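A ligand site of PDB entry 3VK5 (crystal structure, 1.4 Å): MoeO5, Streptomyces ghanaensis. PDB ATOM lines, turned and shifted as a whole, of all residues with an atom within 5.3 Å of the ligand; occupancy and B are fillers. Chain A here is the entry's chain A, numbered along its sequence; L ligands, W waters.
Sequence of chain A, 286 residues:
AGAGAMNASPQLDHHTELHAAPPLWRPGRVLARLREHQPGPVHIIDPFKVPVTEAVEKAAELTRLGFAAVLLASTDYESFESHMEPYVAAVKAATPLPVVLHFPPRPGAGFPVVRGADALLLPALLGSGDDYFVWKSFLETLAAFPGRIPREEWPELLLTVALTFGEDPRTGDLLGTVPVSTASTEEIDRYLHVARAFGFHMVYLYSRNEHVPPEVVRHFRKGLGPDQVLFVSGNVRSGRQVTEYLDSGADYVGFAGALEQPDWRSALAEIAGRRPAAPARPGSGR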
ATOM      1  N   ILE A  44      32.860 -10.390 -16.590  1.00  0.00           N
ATOM      2  CA  ILE A  44      31.975 -11.081 -17.530  1.00  0.00           C
ATOM      3  C   ILE A  44      32.573 -10.873 -18.916  1.00  0.00           C
ATOM      4  O   ILE A  44      32.733  -9.774 -19.376  1.00  0.00           O
ATOM      5  CB  ILE A  44      30.575 -10.453 -17.444  1.00  0.00           C
ATOM      6  CG1 ILE A  44      29.976 -10.595 -16.041  1.00  0.00           C
ATOM      7  CG2 ILE A  44      29.687 -11.099 -18.472  1.00  0.00           C
ATOM      8  CD1 ILE A  44      28.815  -9.583 -15.790  1.00  0.00           C
ATOM      9  N   ALA A  73      28.873 -14.302 -21.015  1.00  0.00           N
ATOM     10  CA  ALA A  73      27.517 -13.854 -21.149  1.00  0.00           C
ATOM     11  C   ALA A  73      27.348 -12.848 -22.234  1.00  0.00           C
ATOM     12  O   ALA A  73      28.241 -12.038 -22.509  1.00  0.00           O
ATOM     13  CB  ALA A  73      27.062 -13.181 -19.809  1.00  0.00           C
ATOM     14  N   SER A  74      26.194 -12.841 -22.881  1.00  0.00           N
ATOM     15  CA  SER A  74      25.886 -11.866 -23.880  1.00  0.00           C
ATOM     16  C   SER A  74      24.391 -11.858 -24.124  1.00  0.00           C
ATOM     17  O   SER A  74      23.728 -12.897 -23.985  1.00  0.00           O
ATOM     18  CB  SER A  74      26.540 -12.215 -25.203  1.00  0.00           C
ATOM     19  OG  SER A  74      26.364 -11.118 -26.101  1.00  0.00           O
ATOM     20  N   THR A  75      23.876 -10.695 -24.545  1.00  0.00           N
ATOM     21  CA  THR A  75      22.509 -10.613 -24.948  1.00  0.00           C
ATOM     22  C   THR A  75      22.366 -11.307 -26.301  1.00  0.00           C
ATOM     23  O   THR A  75      21.357 -11.925 -26.586  1.00  0.00           O
ATOM     24  CB  THR A  75      22.088  -9.143 -25.109  1.00  0.00           C
ATOM     25  OG1 THR A  75      22.239  -8.490 -23.825  1.00  0.00           O
ATOM     26  CG2 THR A  75      20.632  -9.061 -25.573  1.00  0.00           C
ATOM     27  N   HIS A 102      25.711 -17.270 -19.152  1.00  0.00           N
ATOM     28  CA  HIS A 102      24.490 -16.473 -18.909  1.00  0.00           C
ATOM     29  C   HIS A 102      24.031 -15.846 -20.203  1.00  0.00           C
ATOM     30  O   HIS A 102      24.641 -14.903 -20.717  1.00  0.00           O
ATOM     31  CB  HIS A 102      24.758 -15.405 -17.878  1.00  0.00           C
ATOM     32  CG  HIS A 102      23.529 -14.686 -17.446  1.00  0.00           C
ATOM     33  ND1 HIS A 102      23.582 -13.456 -16.824  1.00  0.00           N
ATOM     34  CD2 HIS A 102      22.221 -15.031 -17.516  1.00  0.00           C
ATOM     35  CE1 HIS A 102      22.344 -13.093 -16.501  1.00  0.00           C
ATOM     36  NE2 HIS A 102      21.490 -14.024 -16.904  1.00  0.00           N
ATOM     37  N   PHE A 103      22.959 -16.391 -20.775  1.00  0.00           N
ATOM     38  CA  PHE A 103      22.400 -15.963 -22.050  1.00  0.00           C
ATOM     39  C   PHE A 103      20.859 -16.055 -21.985  1.00  0.00           C
ATOM     40  O   PHE A 103      20.309 -16.874 -21.269  1.00  0.00           O
ATOM     41  CB  PHE A 103      22.875 -16.905 -23.186  1.00  0.00           C
ATOM     42  CG  PHE A 103      24.366 -16.882 -23.376  1.00  0.00           C
ATOM     43  CD1 PHE A 103      25.187 -17.726 -22.647  1.00  0.00           C
ATOM     44  CD2 PHE A 103      24.947 -15.970 -24.250  1.00  0.00           C
ATOM     45  CE1 PHE A 103      26.589 -17.653 -22.779  1.00  0.00           C
ATOM     46  CE2 PHE A 103      26.402 -15.918 -24.371  1.00  0.00           C
ATOM     47  CZ  PHE A 103      27.170 -16.769 -23.629  1.00  0.00           C
ATOM     48  N   PRO A 104      20.186 -15.274 -22.807  1.00  0.00           N
ATOM     49  CA  PRO A 104      18.723 -15.348 -22.812  1.00  0.00           C
ATOM     50  C   PRO A 104      18.241 -16.588 -23.558  1.00  0.00           C
ATOM     51  O   PRO A 104      18.942 -17.180 -24.427  1.00  0.00           O
ATOM     52  CB  PRO A 104      18.283 -14.076 -23.555  1.00  0.00           C
ATOM     53  CG  PRO A 104      19.425 -13.746 -24.444  1.00  0.00           C
ATOM     54  CD  PRO A 104      20.670 -14.123 -23.566  1.00  0.00           C
ATOM     55  N   PRO A 123      18.029 -17.170 -15.887  1.00  0.00           N
ATOM     56  CA  PRO A 123      17.291 -15.984 -15.415  1.00  0.00           C
ATOM     57  C   PRO A 123      15.779 -16.098 -15.604  1.00  0.00           C
ATOM     58  O   PRO A 123      15.308 -16.267 -16.754  1.00  0.00           O
ATOM     59  CB  PRO A 123      17.857 -14.847 -16.308  1.00  0.00           C
ATOM     60  CG  PRO A 123      18.309 -15.516 -17.560  1.00  0.00           C
ATOM     61  CD  PRO A 123      18.811 -16.895 -17.114  1.00  0.00           C
ATOM     62  N   LEU A 125      12.827 -13.833 -15.604  1.00  0.00           N
ATOM     63  CA  LEU A 125      12.701 -12.364 -15.754  1.00  0.00           C
ATOM     64  C   LEU A 125      11.323 -12.015 -15.216  1.00  0.00           C
ATOM     65  O   LEU A 125      10.321 -11.860 -15.943  1.00  0.00           O
ATOM     66  CB  LEU A 125      12.873 -12.005 -17.235  1.00  0.00           C
ATOM     67  CG  LEU A 125      14.330 -12.305 -17.638  1.00  0.00           C
ATOM     68  CD1 LEU A 125      14.448 -12.807 -19.100  1.00  0.00           C
ATOM     69  CD2 LEU A 125      15.161 -11.036 -17.468  1.00  0.00           C
ATOM     70  N   ALA A 162      15.921 -12.518 -12.274  1.00  0.00           N
ATOM     71  CA  ALA A 162      16.658 -11.518 -13.039  1.00  0.00           C
ATOM     72  C   ALA A 162      15.750 -10.313 -13.193  1.00  0.00           C
ATOM     73  O   ALA A 162      14.631 -10.449 -13.737  1.00  0.00           O
ATOM     74  CB  ALA A 162      17.033 -12.124 -14.380  1.00  0.00           C
ATOM     75  N   LEU A 163      16.229  -9.132 -12.822  1.00  0.00           N
ATOM     76  CA  LEU A 163      15.443  -7.893 -12.810  1.00  0.00           C
ATOM     77  C   LEU A 163      16.228  -6.799 -13.488  1.00  0.00           C
ATOM     78  O   LEU A 163      17.453  -6.700 -13.357  1.00  0.00           O
ATOM     79  CB  LEU A 163      15.145  -7.527 -11.345  1.00  0.00           C
ATOM     80  CG  LEU A 163      14.297  -8.547 -10.589  1.00  0.00           C
ATOM     81  CD1 LEU A 163      14.171  -8.046  -9.112  1.00  0.00           C
ATOM     82  CD2 LEU A 163      12.884  -8.707 -11.239  1.00  0.00           C
ATOM     83  N   THR A 164      15.531  -5.976 -14.256  1.00  0.00           N
ATOM     84  CA  THR A 164      16.156  -4.892 -15.010  1.00  0.00           C
ATOM     85  C   THR A 164      15.715  -3.532 -14.516  1.00  0.00           C
ATOM     86  O   THR A 164      14.578  -3.353 -14.118  1.00  0.00           O
ATOM     87  CB  THR A 164      15.846  -4.991 -16.520  1.00  0.00           C
ATOM     88  OG1 THR A 164      14.444  -4.806 -16.813  1.00  0.00           O
ATOM     89  CG2 THR A 164      16.198  -6.363 -17.056  1.00  0.00           C
ATOM     90  N   THR A 171      16.415  -4.767 -24.122  1.00  0.00           N
ATOM     91  CA  THR A 171      15.942  -5.950 -23.444  1.00  0.00           C
ATOM     92  C   THR A 171      14.405  -5.976 -23.474  1.00  0.00           C
ATOM     93  O   THR A 171      13.830  -7.048 -23.494  1.00  0.00           O
ATOM     94  CB  THR A 171      16.442  -5.973 -21.967  1.00  0.00           C
ATOM     95  OG1 THR A 171      17.858  -5.654 -21.918  1.00  0.00           O
ATOM     96  CG2 THR A 171      16.240  -7.337 -21.389  1.00  0.00           C
ATOM     97  N   LEU A 175      13.004  -9.446 -24.686  1.00  0.00           N
ATOM     98  CA  LEU A 175      12.547 -10.333 -23.612  1.00  0.00           C
ATOM     99  C   LEU A 175      11.301  -9.866 -22.890  1.00  0.00           C
ATOM    100  O   LEU A 175      10.808 -10.539 -21.986  1.00  0.00           O
ATOM    101  CB  LEU A 175      13.682 -10.464 -22.560  1.00  0.00           C
ATOM    102  CG  LEU A 175      15.101 -10.704 -23.099  1.00  0.00           C
ATOM    103  CD1 LEU A 175      16.078 -10.811 -21.902  1.00  0.00           C
ATOM    104  CD2 LEU A 175      15.153 -11.979 -23.929  1.00  0.00           C
ATOM    105  N   TYR A 204      19.759 -11.409  -9.650  1.00  0.00           N
ATOM    106  CA  TYR A 204      20.660 -10.663 -10.537  1.00  0.00           C
ATOM    107  C   TYR A 204      19.964  -9.364 -10.900  1.00  0.00           C
ATOM    108  O   TYR A 204      18.927  -9.365 -11.589  1.00  0.00           O
ATOM    109  CB  TYR A 204      20.914 -11.504 -11.803  1.00  0.00           C
ATOM    110  CG  TYR A 204      22.147 -11.148 -12.609  1.00  0.00           C
ATOM    111  CD1 TYR A 204      22.200  -9.987 -13.409  1.00  0.00           C
ATOM    112  CD2 TYR A 204      23.292 -11.943 -12.543  1.00  0.00           C
ATOM    113  CE1 TYR A 204      23.391  -9.645 -14.090  1.00  0.00           C
ATOM    114  CE2 TYR A 204      24.451 -11.589 -13.225  1.00  0.00           C
ATOM    115  CZ  TYR A 204      24.476 -10.460 -13.976  1.00  0.00           C
ATOM    116  OH  TYR A 204      25.638 -10.146 -14.652  1.00  0.00           O
ATOM    117  N   TYR A 206      20.212  -5.918 -12.832  1.00  0.00           N
ATOM    118  CA  TYR A 206      20.954  -5.426 -14.007  1.00  0.00           C
ATOM    119  C   TYR A 206      20.412  -4.135 -14.540  1.00  0.00           C
ATOM    120  O   TYR A 206      19.190  -3.903 -14.511  1.00  0.00           O
ATOM    121  CB  TYR A 206      20.804  -6.503 -15.117  1.00  0.00           C
ATOM    122  CG  TYR A 206      21.231  -6.010 -16.509  1.00  0.00           C
ATOM    123  CD1 TYR A 206      22.544  -5.666 -16.782  1.00  0.00           C
ATOM    124  CD2 TYR A 206      20.303  -5.949 -17.546  1.00  0.00           C
ATOM    125  CE1 TYR A 206      22.957  -5.298 -18.073  1.00  0.00           C
ATOM    126  CE2 TYR A 206      20.678  -5.586 -18.855  1.00  0.00           C
ATOM    127  CZ  TYR A 206      22.003  -5.285 -19.092  1.00  0.00           C
ATOM    128  OH  TYR A 206      22.361  -5.036 -20.416  1.00  0.00           O
ATOM    129  N   SER A 207      21.292  -3.233 -14.963  1.00  0.00           N
ATOM    130  CA  SER A 207      20.834  -2.022 -15.685  1.00  0.00           C
ATOM    131  C   SER A 207      21.671  -1.888 -16.952  1.00  0.00           C
ATOM    132  O   SER A 207      22.908  -1.701 -16.886  1.00  0.00           O
ATOM    133  CB  SER A 207      21.012  -0.774 -14.832  1.00  0.00           C
ATOM    134  OG  SER A 207      20.506   0.336 -15.571  1.00  0.00           O
ATOM    135  N   ARG A 208      21.026  -1.957 -18.100  1.00  0.00           N
ATOM    136  CA  ARG A 208      21.782  -1.806 -19.352  1.00  0.00           C
ATOM    137  C   ARG A 208      22.294  -0.401 -19.546  1.00  0.00           C
ATOM    138  O   ARG A 208      23.489  -0.222 -19.922  1.00  0.00           O
ATOM    139  CB  ARG A 208      20.899  -2.180 -20.572  1.00  0.00           C
ATOM    140  CG  ARG A 208      21.724  -2.217 -21.880  1.00  0.00           C
ATOM    141  CD  ARG A 208      20.881  -2.603 -23.114  1.00  0.00           C
ATOM    142  NE  ARG A 208      20.337  -3.955 -23.001  1.00  0.00           N
ATOM    143  CZ  ARG A 208      21.029  -5.060 -23.318  1.00  0.00           C
ATOM    144  NH1 ARG A 208      22.287  -4.972 -23.765  1.00  0.00           N
ATOM    145  NH2 ARG A 208      20.453  -6.259 -23.148  1.00  0.00           N
ATOM    146  N   SER A 233      24.927  -5.805 -11.778  1.00  0.00           N
ATOM    147  CA  SER A 233      25.820  -5.432 -12.902  1.00  0.00           C
ATOM    148  C   SER A 233      25.180  -4.361 -13.730  1.00  0.00           C
ATOM    149  O   SER A 233      23.939  -4.103 -13.619  1.00  0.00           O
ATOM    150  CB  SER A 233      26.132  -6.646 -13.798  1.00  0.00           C
ATOM    151  OG  SER A 233      25.072  -6.853 -14.695  1.00  0.00           O
ATOM    152  N   GLY A 234      26.007  -3.782 -14.611  1.00  0.00           N
ATOM    153  CA  GLY A 234      25.555  -2.790 -15.561  1.00  0.00           C
ATOM    154  C   GLY A 234      26.250  -1.481 -15.350  1.00  0.00           C
ATOM    155  O   GLY A 234      26.058  -0.844 -14.336  1.00  0.00           O
ATOM    156  N   ASN A 235      27.133  -1.142 -16.277  1.00  0.00           N
ATOM    157  CA  ASN A 235      27.874   0.155 -16.192  1.00  0.00           C
ATOM    158  C   ASN A 235      28.777   0.331 -15.006  1.00  0.00           C
ATOM    159  O   ASN A 235      28.978   1.469 -14.551  1.00  0.00           O
ATOM    160  CB  ASN A 235      26.892   1.322 -16.396  1.00  0.00           C
ATOM    161  CG  ASN A 235      26.181   1.173 -17.662  1.00  0.00           C
ATOM    162  OD1 ASN A 235      26.810   1.106 -18.732  1.00  0.00           O
ATOM    163  ND2 ASN A 235      24.847   1.039 -17.604  1.00  0.00           N
ATOM    164  N   VAL A 236      29.342  -0.751 -14.482  1.00  0.00           N
ATOM    165  CA  VAL A 236      30.333  -0.672 -13.420  1.00  0.00           C
ATOM    166  C   VAL A 236      31.665  -0.488 -14.134  1.00  0.00           C
ATOM    167  O   VAL A 236      32.131  -1.363 -14.874  1.00  0.00           O
ATOM    168  CB  VAL A 236      30.336  -1.966 -12.596  1.00  0.00           C
ATOM    169  CG1 VAL A 236      31.470  -1.941 -11.586  1.00  0.00           C
ATOM    170  CG2 VAL A 236      28.992  -2.131 -11.881  1.00  0.00           C
ATOM    171  N   GLY A 254      29.251  -7.527 -11.188  1.00  0.00           N
ATOM    172  CA  GLY A 254      29.679  -7.891 -12.528  1.00  0.00           C
ATOM    173  C   GLY A 254      30.060  -6.701 -13.396  1.00  0.00           C
ATOM    174  O   GLY A 254      29.551  -5.592 -13.249  1.00  0.00           O
ATOM    175  N   PHE A 255      30.974  -6.955 -14.299  1.00  0.00           N
ATOM    176  CA  PHE A 255      31.425  -5.916 -15.220  1.00  0.00           C
ATOM    177  C   PHE A 255      31.975  -6.555 -16.488  1.00  0.00           C
ATOM    178  O   PHE A 255      32.761  -7.485 -16.406  1.00  0.00           O
ATOM    179  CB  PHE A 255      32.473  -4.928 -14.595  1.00  0.00           C
ATOM    180  CG  PHE A 255      33.777  -5.580 -14.191  1.00  0.00           C
ATOM    181  CD1 PHE A 255      33.850  -6.372 -13.049  1.00  0.00           C
ATOM    182  CD2 PHE A 255      34.929  -5.404 -14.956  1.00  0.00           C
ATOM    183  CE1 PHE A 255      35.058  -6.987 -12.687  1.00  0.00           C
ATOM    184  CE2 PHE A 255      36.133  -6.016 -14.603  1.00  0.00           C
ATOM    185  CZ  PHE A 255      36.201  -6.805 -13.469  1.00  0.00           C
ATOM    186  N   ALA A 256      31.457  -6.100 -17.641  1.00  0.00           N
ATOM    187  CA  ALA A 256      31.933  -6.610 -18.923  1.00  0.00           C
ATOM    188  C   ALA A 256      32.583  -5.502 -19.753  1.00  0.00           C
ATOM    189  O   ALA A 256      33.815  -5.540 -20.009  1.00  0.00           O
ATOM    190  CB  ALA A 256      30.754  -7.258 -19.723  1.00  0.00           C
ATOM    191  N   GLY A 257      31.813  -4.485 -20.110  1.00  0.00           N
ATOM    192  CA  GLY A 257      32.259  -3.459 -21.034  1.00  0.00           C
ATOM    193  C   GLY A 257      33.511  -2.754 -20.637  1.00  0.00           C
ATOM    194  O   GLY A 257      34.294  -2.395 -21.526  1.00  0.00           O
ATOM    195  N   ALA A 258      33.750  -2.546 -19.358  1.00  0.00           N
ATOM    196  CA  ALA A 258      34.966  -1.849 -18.933  1.00  0.00           C
ATOM    197  C   ALA A 258      36.240  -2.497 -19.481  1.00  0.00           C
ATOM    198  O   ALA A 258      37.240  -1.820 -19.675  1.00  0.00           O
ATOM    199  CB  ALA A 258      34.993  -1.867 -17.441  1.00  0.00           C
HETATM  200  P1  LIG L   1      28.396  -3.983 -18.613  1.00  0.00           P
HETATM  201  C1  LIG L   1      24.845  -7.971 -20.579  1.00  0.00           C
HETATM  202  C2  LIG L   1      23.742  -8.267 -19.600  1.00  0.00           C
HETATM  203  C3  LIG L   1      23.397  -9.528 -19.217  1.00  0.00           C
HETATM  204  C4  LIG L   1      22.304  -9.530 -18.228  1.00  0.00           C
HETATM  205  C5  LIG L   1      23.998 -10.832 -19.665  1.00  0.00           C
HETATM  206  C6  LIG L   1      23.191 -11.476 -20.833  1.00  0.00           C
HETATM  207  C7  LIG L   1      21.975 -12.276 -20.332  1.00  0.00           C
HETATM  208  C8  LIG L   1      20.668 -11.967 -20.611  1.00  0.00           C
HETATM  209  C9  LIG L   1      20.226 -10.832 -21.459  1.00  0.00           C
HETATM  210  C10 LIG L   1      27.380  -6.412 -18.020  1.00  0.00           C
HETATM  211  O1  LIG L   1      27.131  -5.055 -18.393  1.00  0.00           O
HETATM  212  C11 LIG L   1      26.125  -7.196 -18.436  1.00  0.00           C
HETATM  213  O2  LIG L   1      25.977  -7.202 -19.800  1.00  0.00           O
HETATM  214  C12 LIG L   1      26.205  -8.554 -17.790  1.00  0.00           C
HETATM  215  C13 LIG L   1      19.600 -12.873 -20.041  1.00  0.00           C
HETATM  216  C14 LIG L   1      18.523 -12.156 -19.231  1.00  0.00           C
HETATM  217  C15 LIG L   1      19.040 -11.564 -17.953  1.00  0.00           C
HETATM  218  C16 LIG L   1      18.945 -10.265 -17.537  1.00  0.00           C
HETATM  219  C17 LIG L   1      18.288  -9.193 -18.380  1.00  0.00           C
HETATM  220  C18 LIG L   1      19.539  -9.892 -16.223  1.00  0.00           C
HETATM  221  O3  LIG L   1      29.406  -4.165 -17.514  1.00  0.00           O
HETATM  222  O4  LIG L   1      25.734  -8.630 -16.611  1.00  0.00           O
HETATM  223  O5  LIG L   1      28.964  -4.242 -19.997  1.00  0.00           O
HETATM  224  O6  LIG L   1      26.681  -9.539 -18.436  1.00  0.00           O
HETATM  225  O7  LIG L   1      27.689  -2.630 -18.486  1.00  0.00           O
HETATM  226  O   HOH W   1      28.728  -3.628 -14.984  1.00  0.00           O
HETATM  227  O   HOH W   2      25.035  -4.584 -20.844  1.00  0.00           O
HETATM  228  O   HOH W   3      31.613  -2.546 -17.369  1.00  0.00           O
HETATM  229  O   HOH W   4      25.509  -2.145 -19.954  1.00  0.00           O
HETATM  230  O   HOH W   5      27.744  -5.913 -21.604  1.00  0.00           O
HETATM  231  O   HOH W   6      26.046 -11.910 -16.800  1.00  0.00           O
HETATM  232  O   HOH W   7      29.960  -0.732 -18.793  1.00  0.00           O
HETATM  233  O   HOH W   8      28.529  -2.394 -21.966  1.00  0.00           O
HETATM  234  O   HOH W   9      27.981  -9.500 -20.999  1.00  0.00           O
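OH of Tyr 204 is in hydrogen-bond range of O4 of the ligand (2.5 Å). The side-chain hydroxyl of Ser 233 is in hydrogen-bond range of an oxygen (O4) of the ligand. The backbone NH (N) of Asn 235 sits at hydrogen-bond distance from an oxygen (O7) of the ligand, at 2.7 Å. An oxygen (O3) of the ligand sits at hydrogen-bond distance from the backbone NH of Ala 256 (2.8 Å). An oxygen (O5) of the ligand is in hydrogen-bond range of the backbone NH (N) of Gly 257 (2.9 Å).
The side-chain hydroxyl (OG) of Ser 233 lies close to the side-chain hydroxyl (OH) of Tyr 204, at 3.3 Å. The backbone NH (N) of Ser 207 is in hydrogen-bond range of the backbone carbonyl oxygen (O) of Ser 233 (3.1 Å). The side-chain amide nitrogen (ND2) of Asn 235 lies within hydrogen-bond range of the backbone carbonyl oxygen (O) of Arg 208 (3.0 Å). ND2 of Asn 235 sits at hydrogen-bond distance from O of Ser 207 (3.4 Å). N of Ile 44 lies within hydrogen-bond range of O of Phe 255, at 2.9 Å. N of Tyr 206 sits at hydrogen-bond distance from O of Leu 163, 2.9 Å away. OH of Tyr 206 sits close to NH1 of Arg 208, 3.4 Å away. O of His 102 is in hydrogen-bond range of N of Ser 74, 3.4 Å away.
Ile 44 touches the ligand. CB of Ala 73 touches C5 of the ligand, at 3.9 Å. O of Ser 74 touches C6 of the ligand, 3.5 Å away. Thr 75 touches the ligand. NE2 of His 102 touches C15 of the ligand (3.6 Å). Phe 103 touches the ligand (C to C13, 3.9 Å). CD of Pro 104 touches C8 of the ligand, at 3.7 Å. Pro 123 touches the ligand (CG to C14, 3.8 Å). CD2 of Leu 125 touches C17 of the ligand (3.7 Å). Ala 162 touches the ligand (CB to C18, 3.8 Å). Thr 164 touches the ligand. Leu 175 touches the ligand (CD1 to C14, 3.9 Å). CE1 of Tyr 206 touches C2 of the ligand, at 3.4 Å. CA of Gly 234 touches O7 of the ligand, at 3.6 Å. CA of Phe 255 touches O3 of the ligand, 3.5 Å away. Hydrophobic or aromatic side chains within 4 Å of the ligand: Ile 44, Ala 73, His 102, Pro 104, Pro 123, Leu 125, Ala 162, Leu 175, Tyr 204, Tyr 206 and Ala 256. 20 residues have an atom within 4 Å of the ligand: Ile 44, Ala 73, Ser 74, Thr 75, His 102, Phe 103, Pro 104, Pro 123, Leu 125, Ala 162, Thr 164, Leu 175, Tyr 204, Tyr 206, Ser 233, Gly 234, Asn 235, Phe 255, Ala 256 and Gly 257.
Water W4 bridges O7 of the ligand (2.7 Å) and O of Arg 208 (2.8 Å). Water W3 lies within hydrogen-bond range of an oxygen (O3) of the ligand (2.7 Å), the backbone carbonyl oxygen (O) of Val 236 (2.8 Å), the backbone NH (N) of Ala 258 (2.9 Å) and the backbone NH (N) of Gly 257 (3.4 Å). Water W9 bridges O6 of the ligand and O of Ala 73. Water W6 lies within hydrogen-bond range of the side-chain hydroxyl (OH) of Tyr 204 (2.8 Å), a ring nitrogen (ND1) of His 102 (2.9 Å) and an oxygen (O6) of the ligand (2.9 Å). Water W2 bridges OH of Tyr 206 (2.7 Å) and O2 of the ligand (3.0 Å).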
